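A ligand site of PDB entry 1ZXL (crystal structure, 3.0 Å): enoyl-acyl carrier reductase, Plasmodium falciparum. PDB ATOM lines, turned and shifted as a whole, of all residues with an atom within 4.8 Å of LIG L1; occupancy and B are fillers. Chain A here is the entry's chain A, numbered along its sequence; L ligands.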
ATOM      1  N   GLY A   8      31.733 -21.867  24.576  1.00  0.00           N
ATOM      2  CA  GLY A   8      31.063 -21.790  23.258  1.00  0.00           C
ATOM      3  C   GLY A   8      30.502 -20.429  22.872  1.00  0.00           C
ATOM      4  O   GLY A   8      29.340 -20.120  23.086  1.00  0.00           O
ATOM      5  N   ILE A   9      31.354 -19.622  22.275  1.00  0.00           N
ATOM      6  CA  ILE A   9      31.034 -18.269  21.871  1.00  0.00           C
ATOM      7  C   ILE A   9      31.989 -17.930  20.719  1.00  0.00           C
ATOM      8  O   ILE A   9      33.133 -18.417  20.676  1.00  0.00           O
ATOM      9  CB  ILE A   9      31.127 -17.285  23.095  1.00  0.00           C
ATOM     10  CG1 ILE A   9      29.862 -17.404  23.934  1.00  0.00           C
ATOM     11  CG2 ILE A   9      31.335 -15.831  22.667  1.00  0.00           C
ATOM     12  CD1 ILE A   9      29.234 -16.072  24.261  1.00  0.00           C
ATOM     13  N   GLY A  10      31.475 -17.161  19.760  1.00  0.00           N
ATOM     14  CA  GLY A  10      32.225 -16.598  18.649  1.00  0.00           C
ATOM     15  C   GLY A  10      31.572 -15.291  18.202  1.00  0.00           C
ATOM     16  O   GLY A  10      32.123 -14.561  17.360  1.00  0.00           O
ATOM     17  N   ASP A  11      30.405 -14.996  18.758  1.00  0.00           N
ATOM     18  CA  ASP A  11      29.679 -13.769  18.467  1.00  0.00           C
ATOM     19  C   ASP A  11      28.646 -13.502  19.564  1.00  0.00           C
ATOM     20  O   ASP A  11      28.693 -14.134  20.616  1.00  0.00           O
ATOM     21  CB  ASP A  11      28.967 -13.877  17.128  1.00  0.00           C
ATOM     22  CG  ASP A  11      28.036 -15.053  17.095  1.00  0.00           C
ATOM     23  OD1 ASP A  11      26.833 -14.856  17.332  1.00  0.00           O
ATOM     24  OD2 ASP A  11      28.536 -16.179  16.877  1.00  0.00           O
ATOM     25  N   GLY A  14      24.157 -15.718  19.545  1.00  0.00           N
ATOM     26  CA  GLY A  14      23.827 -17.041  20.041  1.00  0.00           C
ATOM     27  C   GLY A  14      23.188 -17.104  21.401  1.00  0.00           C
ATOM     28  O   GLY A  14      22.906 -16.093  22.023  1.00  0.00           O
ATOM     29  N   TYR A  15      22.964 -18.321  21.872  1.00  0.00           N
ATOM     30  CA  TYR A  15      22.397 -18.537  23.191  1.00  0.00           C
ATOM     31  C   TYR A  15      23.349 -18.277  24.352  1.00  0.00           C
ATOM     32  O   TYR A  15      22.907 -17.916  25.433  1.00  0.00           O
ATOM     33  CB  TYR A  15      21.800 -19.942  23.270  1.00  0.00           C
ATOM     34  CG  TYR A  15      20.448 -20.104  22.599  1.00  0.00           C
ATOM     35  CD1 TYR A  15      19.362 -19.284  22.945  1.00  0.00           C
ATOM     36  CD2 TYR A  15      20.234 -21.076  21.619  1.00  0.00           C
ATOM     37  CE1 TYR A  15      18.112 -19.423  22.326  1.00  0.00           C
ATOM     38  CE2 TYR A  15      18.969 -21.233  21.002  1.00  0.00           C
ATOM     39  CZ  TYR A  15      17.911 -20.398  21.363  1.00  0.00           C
ATOM     40  OH  TYR A  15      16.676 -20.521  20.764  1.00  0.00           O
ATOM     41  N   GLY A  16      24.652 -18.470  24.164  1.00  0.00           N
ATOM     42  CA  GLY A  16      25.635 -18.238  25.224  1.00  0.00           C
ATOM     43  C   GLY A  16      25.567 -16.797  25.655  1.00  0.00           C
ATOM     44  O   GLY A  16      25.534 -16.470  26.851  1.00  0.00           O
ATOM     45  N   TRP A  35      36.109 -20.355  20.960  1.00  0.00           N
ATOM     46  CA  TRP A  35      36.770 -21.281  20.051  1.00  0.00           C
ATOM     47  C   TRP A  35      37.980 -20.552  19.494  1.00  0.00           C
ATOM     48  O   TRP A  35      37.843 -19.418  19.029  1.00  0.00           O
ATOM     49  CB  TRP A  35      35.799 -21.626  18.927  1.00  0.00           C
ATOM     50  CG  TRP A  35      36.214 -22.713  18.013  1.00  0.00           C
ATOM     51  CD1 TRP A  35      36.816 -23.886  18.351  1.00  0.00           C
ATOM     52  CD2 TRP A  35      35.985 -22.771  16.611  1.00  0.00           C
ATOM     53  NE1 TRP A  35      37.017 -24.659  17.239  1.00  0.00           N
ATOM     54  CE2 TRP A  35      36.513 -24.002  16.148  1.00  0.00           C
ATOM     55  CE3 TRP A  35      35.404 -21.897  15.666  1.00  0.00           C
ATOM     56  CZ2 TRP A  35      36.479 -24.389  14.789  1.00  0.00           C
ATOM     57  CZ3 TRP A  35      35.366 -22.266  14.320  1.00  0.00           C
ATOM     58  CH2 TRP A  35      35.896 -23.504  13.901  1.00  0.00           C
ATOM     59  N   VAL A  38      38.263 -18.217  16.227  1.00  0.00           N
ATOM     60  CA  VAL A  38      37.639 -16.880  16.210  1.00  0.00           C
ATOM     61  C   VAL A  38      37.942 -16.018  17.443  1.00  0.00           C
ATOM     62  O   VAL A  38      37.462 -14.886  17.549  1.00  0.00           O
ATOM     63  CB  VAL A  38      36.116 -16.911  15.953  1.00  0.00           C
ATOM     64  CG1 VAL A  38      35.791 -17.772  14.721  1.00  0.00           C
ATOM     65  CG2 VAL A  38      35.359 -17.391  17.183  1.00  0.00           C
ATOM     66  N   PHE A  71      39.382 -21.296  24.100  1.00  0.00           N
ATOM     67  CA  PHE A  71      38.911 -22.556  24.658  1.00  0.00           C
ATOM     68  C   PHE A  71      38.498 -23.475  23.522  1.00  0.00           C
ATOM     69  O   PHE A  71      37.743 -23.066  22.649  1.00  0.00           O
ATOM     70  CB  PHE A  71      37.719 -22.309  25.587  1.00  0.00           C
ATOM     71  CG  PHE A  71      36.950 -23.559  25.926  1.00  0.00           C
ATOM     72  CD1 PHE A  71      37.426 -24.445  26.875  1.00  0.00           C
ATOM     73  CD2 PHE A  71      35.737 -23.841  25.296  1.00  0.00           C
ATOM     74  CE1 PHE A  71      36.722 -25.603  27.177  1.00  0.00           C
ATOM     75  CE2 PHE A  71      35.014 -25.006  25.588  1.00  0.00           C
ATOM     76  CZ  PHE A  71      35.509 -25.881  26.525  1.00  0.00           C
ATOM     77  N   ASP A  72      38.983 -24.695  23.519  1.00  0.00           N
ATOM     78  CA  ASP A  72      38.685 -25.598  22.407  1.00  0.00           C
ATOM     79  C   ASP A  72      38.222 -26.952  22.913  1.00  0.00           C
ATOM     80  O   ASP A  72      39.000 -27.734  23.439  1.00  0.00           O
ATOM     81  CB  ASP A  72      39.874 -25.747  21.443  1.00  0.00           C
ATOM     82  CG  ASP A  72      39.506 -26.450  20.142  1.00  0.00           C
ATOM     83  OD1 ASP A  72      38.511 -27.207  20.130  1.00  0.00           O
ATOM     84  OD2 ASP A  72      40.214 -26.266  19.133  1.00  0.00           O
ATOM     85  N   ALA A  73      36.930 -27.194  22.708  1.00  0.00           N
ATOM     86  CA  ALA A  73      36.231 -28.320  23.251  1.00  0.00           C
ATOM     87  C   ALA A  73      36.656 -29.683  22.655  1.00  0.00           C
ATOM     88  O   ALA A  73      36.234 -30.741  23.128  1.00  0.00           O
ATOM     89  CB  ALA A  73      34.777 -28.084  23.059  1.00  0.00           C
ATOM     90  N   SER A  74      37.508 -29.663  21.639  1.00  0.00           N
ATOM     91  CA  SER A  74      37.913 -30.899  20.959  1.00  0.00           C
ATOM     92  C   SER A  74      39.142 -31.569  21.560  1.00  0.00           C
ATOM     93  O   SER A  74      39.393 -32.755  21.281  1.00  0.00           O
ATOM     94  CB  SER A  74      38.098 -30.681  19.456  1.00  0.00           C
ATOM     95  OG  SER A  74      39.052 -29.676  19.210  1.00  0.00           O
ATOM     96  N   SER A 119      27.548 -24.587  25.938  1.00  0.00           N
ATOM     97  CA  SER A 119      26.718 -23.993  24.906  1.00  0.00           C
ATOM     98  C   SER A 119      27.389 -24.032  23.539  1.00  0.00           C
ATOM     99  O   SER A 119      27.611 -23.000  22.888  1.00  0.00           O
ATOM    100  CB  SER A 119      26.337 -22.581  25.306  1.00  0.00           C
ATOM    101  OG  SER A 119      25.800 -21.879  24.205  1.00  0.00           O
ATOM    102  N   LEU A 120      27.723 -25.236  23.074  1.00  0.00           N
ATOM    103  CA  LEU A 120      28.463 -25.354  21.842  1.00  0.00           C
ATOM    104  C   LEU A 120      28.063 -26.571  21.033  1.00  0.00           C
ATOM    105  O   LEU A 120      27.664 -27.596  21.611  1.00  0.00           O
ATOM    106  CB  LEU A 120      29.964 -25.389  22.148  1.00  0.00           C
ATOM    107  CG  LEU A 120      30.660 -26.635  22.690  1.00  0.00           C
ATOM    108  CD1 LEU A 120      31.359 -27.354  21.556  1.00  0.00           C
ATOM    109  CD2 LEU A 120      31.663 -26.197  23.729  1.00  0.00           C
ATOM    110  N   ALA A 121      28.173 -26.457  19.704  1.00  0.00           N
ATOM    111  CA  ALA A 121      27.990 -27.604  18.785  1.00  0.00           C
ATOM    112  C   ALA A 121      28.830 -27.532  17.524  1.00  0.00           C
ATOM    113  O   ALA A 121      29.071 -26.462  16.943  1.00  0.00           O
ATOM    114  CB  ALA A 121      26.528 -27.795  18.415  1.00  0.00           C
ATOM    115  N   ASN A 122      29.265 -28.719  17.088  1.00  0.00           N
ATOM    116  CA  ASN A 122      29.918 -28.902  15.806  1.00  0.00           C
ATOM    117  C   ASN A 122      29.618 -30.284  15.204  1.00  0.00           C
ATOM    118  O   ASN A 122      29.705 -31.323  15.858  1.00  0.00           O
ATOM    119  CB  ASN A 122      31.428 -28.680  15.891  1.00  0.00           C
ATOM    120  CG  ASN A 122      31.953 -27.747  14.816  1.00  0.00           C
ATOM    121  OD1 ASN A 122      32.965 -27.075  15.027  1.00  0.00           O
ATOM    122  ND2 ASN A 122      31.274 -27.688  13.680  1.00  0.00           N
ATOM    123  N   LYS A 144      32.849 -33.410  19.555  1.00  0.00           N
ATOM    124  CA  LYS A 144      32.745 -31.995  19.788  1.00  0.00           C
ATOM    125  C   LYS A 144      31.453 -31.568  20.467  1.00  0.00           C
ATOM    126  O   LYS A 144      31.492 -30.669  21.298  1.00  0.00           O
ATOM    127  CB  LYS A 144      33.016 -31.237  18.480  1.00  0.00           C
ATOM    128  CG  LYS A 144      34.436 -31.480  17.974  1.00  0.00           C
ATOM    129  CD  LYS A 144      34.807 -30.537  16.848  1.00  0.00           C
ATOM    130  CE  LYS A 144      36.231 -30.761  16.413  1.00  0.00           C
ATOM    131  NZ  LYS A 144      36.461 -29.926  15.218  1.00  0.00           N
ATOM    132  N   LEU A 169      22.863 -26.911  26.258  1.00  0.00           N
ATOM    133  CA  LEU A 169      21.754 -26.650  25.353  1.00  0.00           C
ATOM    134  C   LEU A 169      21.511 -27.819  24.413  1.00  0.00           C
ATOM    135  O   LEU A 169      22.449 -28.400  23.868  1.00  0.00           O
ATOM    136  CB  LEU A 169      22.062 -25.390  24.570  1.00  0.00           C
ATOM    137  CG  LEU A 169      21.538 -24.039  25.039  1.00  0.00           C
ATOM    138  CD1 LEU A 169      21.317 -23.972  26.504  1.00  0.00           C
ATOM    139  CD2 LEU A 169      22.544 -23.013  24.642  1.00  0.00           C
ATOM    140  N   THR A 170      20.251 -28.174  24.198  1.00  0.00           N
ATOM    141  CA  THR A 170      19.938 -29.340  23.338  1.00  0.00           C
ATOM    142  C   THR A 170      18.886 -28.989  22.292  1.00  0.00           C
ATOM    143  O   THR A 170      18.380 -27.867  22.284  1.00  0.00           O
ATOM    144  CB  THR A 170      19.547 -30.602  24.180  1.00  0.00           C
ATOM    145  OG1 THR A 170      19.327 -31.722  23.303  1.00  0.00           O
ATOM    146  CG2 THR A 170      18.295 -30.347  25.026  1.00  0.00           C
ATOM    147  N   TYR A 171      18.586 -29.938  21.408  1.00  0.00           N
ATOM    148  CA  TYR A 171      17.501 -29.738  20.429  1.00  0.00           C
ATOM    149  C   TYR A 171      16.607 -30.968  20.274  1.00  0.00           C
ATOM    150  O   TYR A 171      17.091 -32.123  20.368  1.00  0.00           O
ATOM    151  CB  TYR A 171      18.073 -29.281  19.062  1.00  0.00           C
ATOM    152  CG  TYR A 171      17.009 -28.875  18.062  1.00  0.00           C
ATOM    153  CD1 TYR A 171      15.981 -28.002  18.421  1.00  0.00           C
ATOM    154  CD2 TYR A 171      17.035 -29.357  16.755  1.00  0.00           C
ATOM    155  CE1 TYR A 171      15.006 -27.628  17.505  1.00  0.00           C
ATOM    156  CE2 TYR A 171      16.038 -28.978  15.818  1.00  0.00           C
ATOM    157  CZ  TYR A 171      15.046 -28.113  16.215  1.00  0.00           C
ATOM    158  OH  TYR A 171      14.050 -27.745  15.343  1.00  0.00           O
ATOM    159  N   TYR A 181      18.362 -31.870   9.911  1.00  0.00           N
ATOM    160  CA  TYR A 181      19.245 -31.799  11.082  1.00  0.00           C
ATOM    161  C   TYR A 181      20.260 -32.934  11.022  1.00  0.00           C
ATOM    162  O   TYR A 181      20.233 -33.848  11.847  1.00  0.00           O
ATOM    163  CB  TYR A 181      18.432 -31.831  12.395  1.00  0.00           C
ATOM    164  CG  TYR A 181      19.185 -31.340  13.610  1.00  0.00           C
ATOM    165  CD1 TYR A 181      19.483 -29.988  13.772  1.00  0.00           C
ATOM    166  CD2 TYR A 181      19.604 -32.229  14.610  1.00  0.00           C
ATOM    167  CE1 TYR A 181      20.194 -29.540  14.894  1.00  0.00           C
ATOM    168  CE2 TYR A 181      20.311 -31.781  15.741  1.00  0.00           C
ATOM    169  CZ  TYR A 181      20.593 -30.442  15.860  1.00  0.00           C
ATOM    170  OH  TYR A 181      21.258 -29.996  16.960  1.00  0.00           O
ATOM    171  N   MET A 185      24.199 -34.747  14.298  1.00  0.00           N
ATOM    172  CA  MET A 185      23.804 -33.849  15.366  1.00  0.00           C
ATOM    173  C   MET A 185      22.676 -34.495  16.185  1.00  0.00           C
ATOM    174  O   MET A 185      22.762 -34.589  17.410  1.00  0.00           O
ATOM    175  CB  MET A 185      23.342 -32.494  14.838  1.00  0.00           C
ATOM    176  CG  MET A 185      24.410 -31.410  14.735  1.00  0.00           C
ATOM    177  SD  MET A 185      25.394 -31.030  16.205  1.00  0.00           S
ATOM    178  CE  MET A 185      24.166 -31.018  17.468  1.00  0.00           C
ATOM    179  N   LYS A 189      22.901 -34.985  20.031  1.00  0.00           N
ATOM    180  CA  LYS A 189      22.057 -34.409  21.067  1.00  0.00           C
ATOM    181  C   LYS A 189      21.363 -35.476  21.933  1.00  0.00           C
ATOM    182  O   LYS A 189      21.220 -35.295  23.147  1.00  0.00           O
ATOM    183  CB  LYS A 189      21.059 -33.436  20.480  1.00  0.00           C
ATOM    184  CG  LYS A 189      21.664 -32.180  19.874  1.00  0.00           C
ATOM    185  CD  LYS A 189      22.522 -31.468  20.865  1.00  0.00           C
ATOM    186  CE  LYS A 189      22.698 -29.999  20.490  1.00  0.00           C
ATOM    187  NZ  LYS A 189      23.786 -29.303  21.266  1.00  0.00           N
ATOM    188  N   ALA A 216      15.949 -26.080  23.271  1.00  0.00           N
ATOM    189  CA  ALA A 216      15.699 -24.717  22.768  1.00  0.00           C
ATOM    190  C   ALA A 216      14.933 -24.672  21.455  1.00  0.00           C
ATOM    191  O   ALA A 216      15.136 -25.527  20.601  1.00  0.00           O
ATOM    192  CB  ALA A 216      16.994 -23.982  22.632  1.00  0.00           C
ATOM    193  N   GLY A 217      14.072 -23.670  21.306  1.00  0.00           N
ATOM    194  CA  GLY A 217      13.427 -23.407  20.023  1.00  0.00           C
ATOM    195  C   GLY A 217      14.457 -22.868  19.043  1.00  0.00           C
ATOM    196  O   GLY A 217      15.633 -22.769  19.376  1.00  0.00           O
ATOM    197  N   PRO A 218      14.024 -22.511  17.816  1.00  0.00           N
ATOM    198  CA  PRO A 218      15.044 -22.094  16.840  1.00  0.00           C
ATOM    199  C   PRO A 218      15.346 -20.615  16.963  1.00  0.00           C
ATOM    200  O   PRO A 218      14.450 -19.792  17.189  1.00  0.00           O
ATOM    201  CB  PRO A 218      14.383 -22.399  15.491  1.00  0.00           C
ATOM    202  CG  PRO A 218      12.937 -22.794  15.807  1.00  0.00           C
ATOM    203  CD  PRO A 218      12.675 -22.445  17.241  1.00  0.00           C
ATOM    204  N   LEU A 219      16.614 -20.277  16.844  1.00  0.00           N
ATOM    205  CA  LEU A 219      17.047 -18.883  16.920  1.00  0.00           C
ATOM    206  C   LEU A 219      17.974 -18.660  15.741  1.00  0.00           C
ATOM    207  O   LEU A 219      18.796 -19.532  15.418  1.00  0.00           O
ATOM    208  CB  LEU A 219      17.801 -18.629  18.218  1.00  0.00           C
ATOM    209  CG  LEU A 219      18.236 -17.204  18.544  1.00  0.00           C
ATOM    210  CD1 LEU A 219      17.065 -16.304  19.004  1.00  0.00           C
ATOM    211  CD2 LEU A 219      19.317 -17.255  19.606  1.00  0.00           C
ATOM    212  N   SER A 221      20.763 -17.666  15.039  1.00  0.00           N
ATOM    213  CA  SER A 221      22.170 -17.442  15.420  1.00  0.00           C
ATOM    214  C   SER A 221      23.087 -17.549  14.219  1.00  0.00           C
ATOM    215  O   SER A 221      22.681 -18.023  13.151  1.00  0.00           O
ATOM    216  CB  SER A 221      22.602 -18.427  16.503  1.00  0.00           C
ATOM    217  OG  SER A 221      22.723 -19.735  15.980  1.00  0.00           O
ATOM    218  N   ARG A 222      24.326 -17.103  14.390  1.00  0.00           N
ATOM    219  CA  ARG A 222      25.341 -17.223  13.335  1.00  0.00           C
ATOM    220  C   ARG A 222      25.518 -18.698  12.874  1.00  0.00           C
ATOM    221  O   ARG A 222      25.706 -18.948  11.683  1.00  0.00           O
ATOM    222  CB  ARG A 222      26.674 -16.556  13.790  1.00  0.00           C
ATOM    223  CG  ARG A 222      27.848 -16.543  12.772  1.00  0.00           C
ATOM    224  CD  ARG A 222      28.819 -17.735  13.029  1.00  0.00           C
ATOM    225  NE  ARG A 222      29.689 -18.050  11.880  1.00  0.00           N
ATOM    226  CZ  ARG A 222      30.129 -19.284  11.608  1.00  0.00           C
ATOM    227  NH1 ARG A 222      29.786 -20.305  12.381  1.00  0.00           N
ATOM    228  NH2 ARG A 222      30.921 -19.485  10.548  1.00  0.00           N
ATOM    229  N   ALA A 223      25.424 -19.645  13.808  1.00  0.00           N
ATOM    230  CA  ALA A 223      25.637 -21.054  13.484  1.00  0.00           C
ATOM    231  C   ALA A 223      24.471 -21.736  12.784  1.00  0.00           C
ATOM    232  O   ALA A 223      24.666 -22.634  11.954  1.00  0.00           O
ATOM    233  CB  ALA A 223      26.024 -21.829  14.738  1.00  0.00           C
ATOM    234  N   ALA A 224      23.253 -21.318  13.107  1.00  0.00           N
ATOM    235  CA  ALA A 224      22.032 -21.880  12.518  1.00  0.00           C
ATOM    236  C   ALA A 224      21.918 -21.490  11.047  1.00  0.00           C
ATOM    237  O   ALA A 224      21.467 -22.272  10.210  1.00  0.00           O
ATOM    238  CB  ALA A 224      20.820 -21.435  13.294  1.00  0.00           C
ATOM    239  N   ILE A 273      16.874 -22.935   9.078  1.00  0.00           N
ATOM    240  CA  ILE A 273      16.629 -22.187  10.301  1.00  0.00           C
ATOM    241  C   ILE A 273      15.528 -21.172  10.071  1.00  0.00           C
ATOM    242  O   ILE A 273      14.700 -20.958  10.949  1.00  0.00           O
ATOM    243  CB  ILE A 273      17.917 -21.538  10.821  1.00  0.00           C
ATOM    244  CG1 ILE A 273      17.640 -20.834  12.146  1.00  0.00           C
ATOM    245  CG2 ILE A 273      18.503 -20.591   9.811  1.00  0.00           C
ATOM    246  CD1 ILE A 273      17.266 -21.790  13.224  1.00  0.00           C
HETATM  247  P1  LIG L   1      26.617 -20.375  18.003  1.00  0.00           P
HETATM  248  O1  LIG L   1      27.313 -20.177  16.664  1.00  0.00           O
HETATM  249  O2  LIG L   1      26.643 -19.263  19.031  1.00  0.00           O
HETATM  250  O3  LIG L   1      27.242 -21.609  18.825  1.00  0.00           O
HETATM  251  C1  LIG L   1      28.275 -22.417  18.309  1.00  0.00           C
HETATM  252  C2  LIG L   1      29.494 -21.929  19.045  1.00  0.00           C
HETATM  253  O4  LIG L   1      30.289 -23.053  19.415  1.00  0.00           O
HETATM  254  C3  LIG L   1      30.316 -21.072  18.093  1.00  0.00           C
HETATM  255  O5  LIG L   1      30.846 -19.942  18.809  1.00  0.00           O
HETATM  256  C4  LIG L   1      31.452 -21.960  17.640  1.00  0.00           C
HETATM  257  O6  LIG L   1      32.582 -21.140  17.312  1.00  0.00           O
HETATM  258  C5  LIG L   1      31.605 -22.801  18.919  1.00  0.00           C
HETATM  259  N1  LIG L   1      32.413 -24.042  18.812  1.00  0.00           N
HETATM  260  C6  LIG L   1      32.321 -25.025  17.901  1.00  0.00           C
HETATM  261  N2  LIG L   1      33.248 -25.981  18.165  1.00  0.00           N
HETATM  262  C7  LIG L   1      33.947 -25.608  19.262  1.00  0.00           C
HETATM  263  C8  LIG L   1      34.983 -26.115  20.024  1.00  0.00           C
HETATM  264  N3  LIG L   1      35.556 -27.291  19.700  1.00  0.00           N
HETATM  265  N4  LIG L   1      35.410 -25.430  21.094  1.00  0.00           N
HETATM  266  C9  LIG L   1      34.883 -24.255  21.462  1.00  0.00           C
HETATM  267  N5  LIG L   1      33.873 -23.684  20.787  1.00  0.00           N
HETATM  268  C10 LIG L   1      33.377 -24.317  19.690  1.00  0.00           C
HETATM  269  O7  LIG L   1      25.071 -20.891  17.798  1.00  0.00           O
HETATM  270  P2  LIG L   1      23.980 -21.252  18.971  1.00  0.00           P
HETATM  271  O8  LIG L   1      22.662 -21.532  18.257  1.00  0.00           O
HETATM  272  O9  LIG L   1      24.136 -20.228  20.096  1.00  0.00           O
HETATM  273  O10 LIG L   1      24.412 -22.680  19.587  1.00  0.00           O
HETATM  274  C11 LIG L   1      24.508 -22.837  21.010  1.00  0.00           C
HETATM  275  C12 LIG L   1      23.888 -24.164  21.433  1.00  0.00           C
HETATM  276  O11 LIG L   1      22.451 -24.091  21.364  1.00  0.00           O
HETATM  277  C13 LIG L   1      24.326 -25.318  20.544  1.00  0.00           C
HETATM  278  O12 LIG L   1      24.684 -26.445  21.352  1.00  0.00           O
HETATM  279  C14 LIG L   1      23.089 -25.660  19.729  1.00  0.00           C
HETATM  280  O13 LIG L   1      23.147 -27.060  19.431  1.00  0.00           O
HETATM  281  C15 LIG L   1      21.925 -25.230  20.638  1.00  0.00           C
HETATM  282  N6  LIG L   1      20.643 -24.864  19.997  1.00  0.00           N
HETATM  283  C16 LIG L   1      20.538 -23.847  19.109  1.00  0.00           C
HETATM  284  C17 LIG L   1      19.310 -23.503  18.514  1.00  0.00           C
HETATM  285  C18 LIG L   1      19.182 -22.381  17.493  1.00  0.00           C
HETATM  286  O14 LIG L   1      18.463 -22.558  16.388  1.00  0.00           O
HETATM  287  N7  LIG L   1      19.741 -21.244  17.643  1.00  0.00           N
HETATM  288  C19 LIG L   1      18.192 -24.247  18.867  1.00  0.00           C
HETATM  289  C20 LIG L   1      18.304 -25.289  19.779  1.00  0.00           C
HETATM  290  C21 LIG L   1      19.546 -25.568  20.343  1.00  0.00           C
HETATM  291  C1  LG2 L   2      21.656 -25.663  16.112  1.00  0.00           C
HETATM  292  C2  LG2 L   2      21.111 -24.702  15.239  1.00  0.00           C
HETATM  293  C3  LG2 L   2      19.747 -24.652  14.956  1.00  0.00           C
HETATM  294  C4  LG2 L   2      18.906 -25.554  15.570  1.00  0.00           C
HETATM  295  C5  LG2 L   2      23.955 -25.944  15.377  1.00  0.00           C
HETATM  296  C6  LG2 L   2      25.246 -25.527  15.570  1.00  0.00           C
HETATM  297  C7  LG2 L   2      26.246 -25.689  14.603  1.00  0.00           C
HETATM  298  C8  LG2 L   2      23.627 -26.567  14.184  1.00  0.00           C
HETATM  299  C9  LG2 L   2      28.082 -26.742  12.412  1.00  0.00           C
HETATM  300  C10 LG2 L   2      30.954 -26.807  10.417  1.00  0.00           C
HETATM  301  C11 LG2 L   2      29.284 -25.678   9.100  1.00  0.00           C
HETATM  302  C12 LG2 L   2      28.241 -25.647  10.209  1.00  0.00           C
HETATM  303  O1  LG2 L   2      28.556 -27.414  13.297  1.00  0.00           O
HETATM  304  N1  LG2 L   2      28.831 -26.182  11.445  1.00  0.00           N
HETATM  305  O2  LG2 L   2      30.138 -26.821   9.240  1.00  0.00           O
HETATM  306  C13 LG2 L   2      30.287 -26.029  11.551  1.00  0.00           C
HETATM  307  N2  LG2 L   2      26.764 -26.531  12.372  1.00  0.00           N
HETATM  308  C14 LG2 L   2      25.910 -26.310  13.405  1.00  0.00           C
HETATM  309 CL1  LG2 L   2      25.565 -24.752  17.146  1.00  0.00          CL
HETATM  310  C15 LG2 L   2      24.604 -26.737  13.216  1.00  0.00           C
HETATM  311  O3  LG2 L   2      23.013 -25.731  16.378  1.00  0.00           O
HETATM  312  C16 LG2 L   2      20.779 -26.559  16.709  1.00  0.00           C
HETATM  313  O4  LG2 L   2      21.229 -27.520  17.569  1.00  0.00           O
HETATM  314  C17 LG2 L   2      19.420 -26.501  16.441  1.00  0.00           C
HETATM  315 CL2  LG2 L   2      17.138 -25.562  15.298  1.00  0.00          CL
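Residues that only touch LIG L1: Gly 14 (3.2 Å), Trp 35 (3.3 Å), Phe 71 (3.3 Å), Ser 74 (3.6 Å), Ser 119 (3.6 Å), Ala 121 (3.6 Å), Leu 169 (3.5 Å), Thr 170 (3.2 Å), Tyr 171 (3.8 Å), Ala 216 (3.3 Å), Gly 217 (3.0 Å), Pro 218 (3.5 Å) and Ile 273 (3.5 Å). Hydrophobic or aromatic side chains that line LIG L1: Tyr 15, Trp 35, Phe 71, Ala 73, Leu 120, Ala 121, Leu 169, Tyr 171, Ala 216, Leu 219, Ala 223 and Ile 273. The nearest printed residue that does not touch LIG L1 is Ala 224 (4.05 Å).
A nitrogen (N4) of LIG L1 is in hydrogen-bond range of the backbone NH (N) of Ala 73 (2.8 Å). An oxygen (O1) of LIG L1 lies close to the backbone NH of Ala 223. The backbone NH (N) of Tyr 15 is in hydrogen-bond range of an oxygen (O9) of LIG L1, at 2.9 Å. The side-chain hydroxyl (OG) of Ser 221 is in hydrogen-bond range of an oxygen (O8) of LIG L1 (2.9 Å). An oxygen (O14) of LIG L1 sits at hydrogen-bond distance from the backbone NH (N) of Leu 219 (3.0 Å). The backbone carbonyl oxygen (O) of Leu 219 lies within hydrogen-bond range of a nitrogen (N7) of LIG L1. NZ of Lys 189 lies within hydrogen-bond range of O13 of LIG L1 (3.0 Å). OD1 of Asp 72 is in hydrogen-bond range of N3 of LIG L1 (3.0 Å). O of Ile 9 sits close to O5 of LIG L1 (3.3 Å). The backbone NH of Gly 10 lies within hydrogen-bond range of an oxygen (O5) of LIG L1. The backbone carbonyl oxygen (O) of Leu 120 sits at hydrogen-bond distance from an oxygen (O12) of LIG L1. OD1 of Asn 122 sits close to N2 of LIG L1, at 3.3 Å. The side-chain amide nitrogen (ND2) of Asn 122 sits at hydrogen-bond distance from an oxygen (O1) of LG2 L2, 2.8 Å away. OH of Tyr 181 sits at hydrogen-bond distance from O4 of LG2 L2, 2.5 Å away.
An oxygen (O13) of LIG L1 lies within hydrogen-bond range of an oxygen (O4) of LG2 L2 (2.7 Å).
N of Ala 223 sits close to OG of Ser 221, 3.5 Å away. The side-chain hydroxyl of Tyr 15 sits at hydrogen-bond distance from the backbone carbonyl oxygen of Gly 217. The side-chain hydroxyl of Ser 221 lies within hydrogen-bond range of the backbone NH of Ala 224 (3.3 Å). NZ of Lys 189 is in hydrogen-bond range of O of Leu 169, at 3.1 Å. OD1 of Asp 72 lies within hydrogen-bond range of OG of Ser 74 (2.7 Å). The backbone NH (N) of Ala 216 is in hydrogen-bond range of the backbone carbonyl oxygen (O) of Thr 170, 3.2 Å away.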
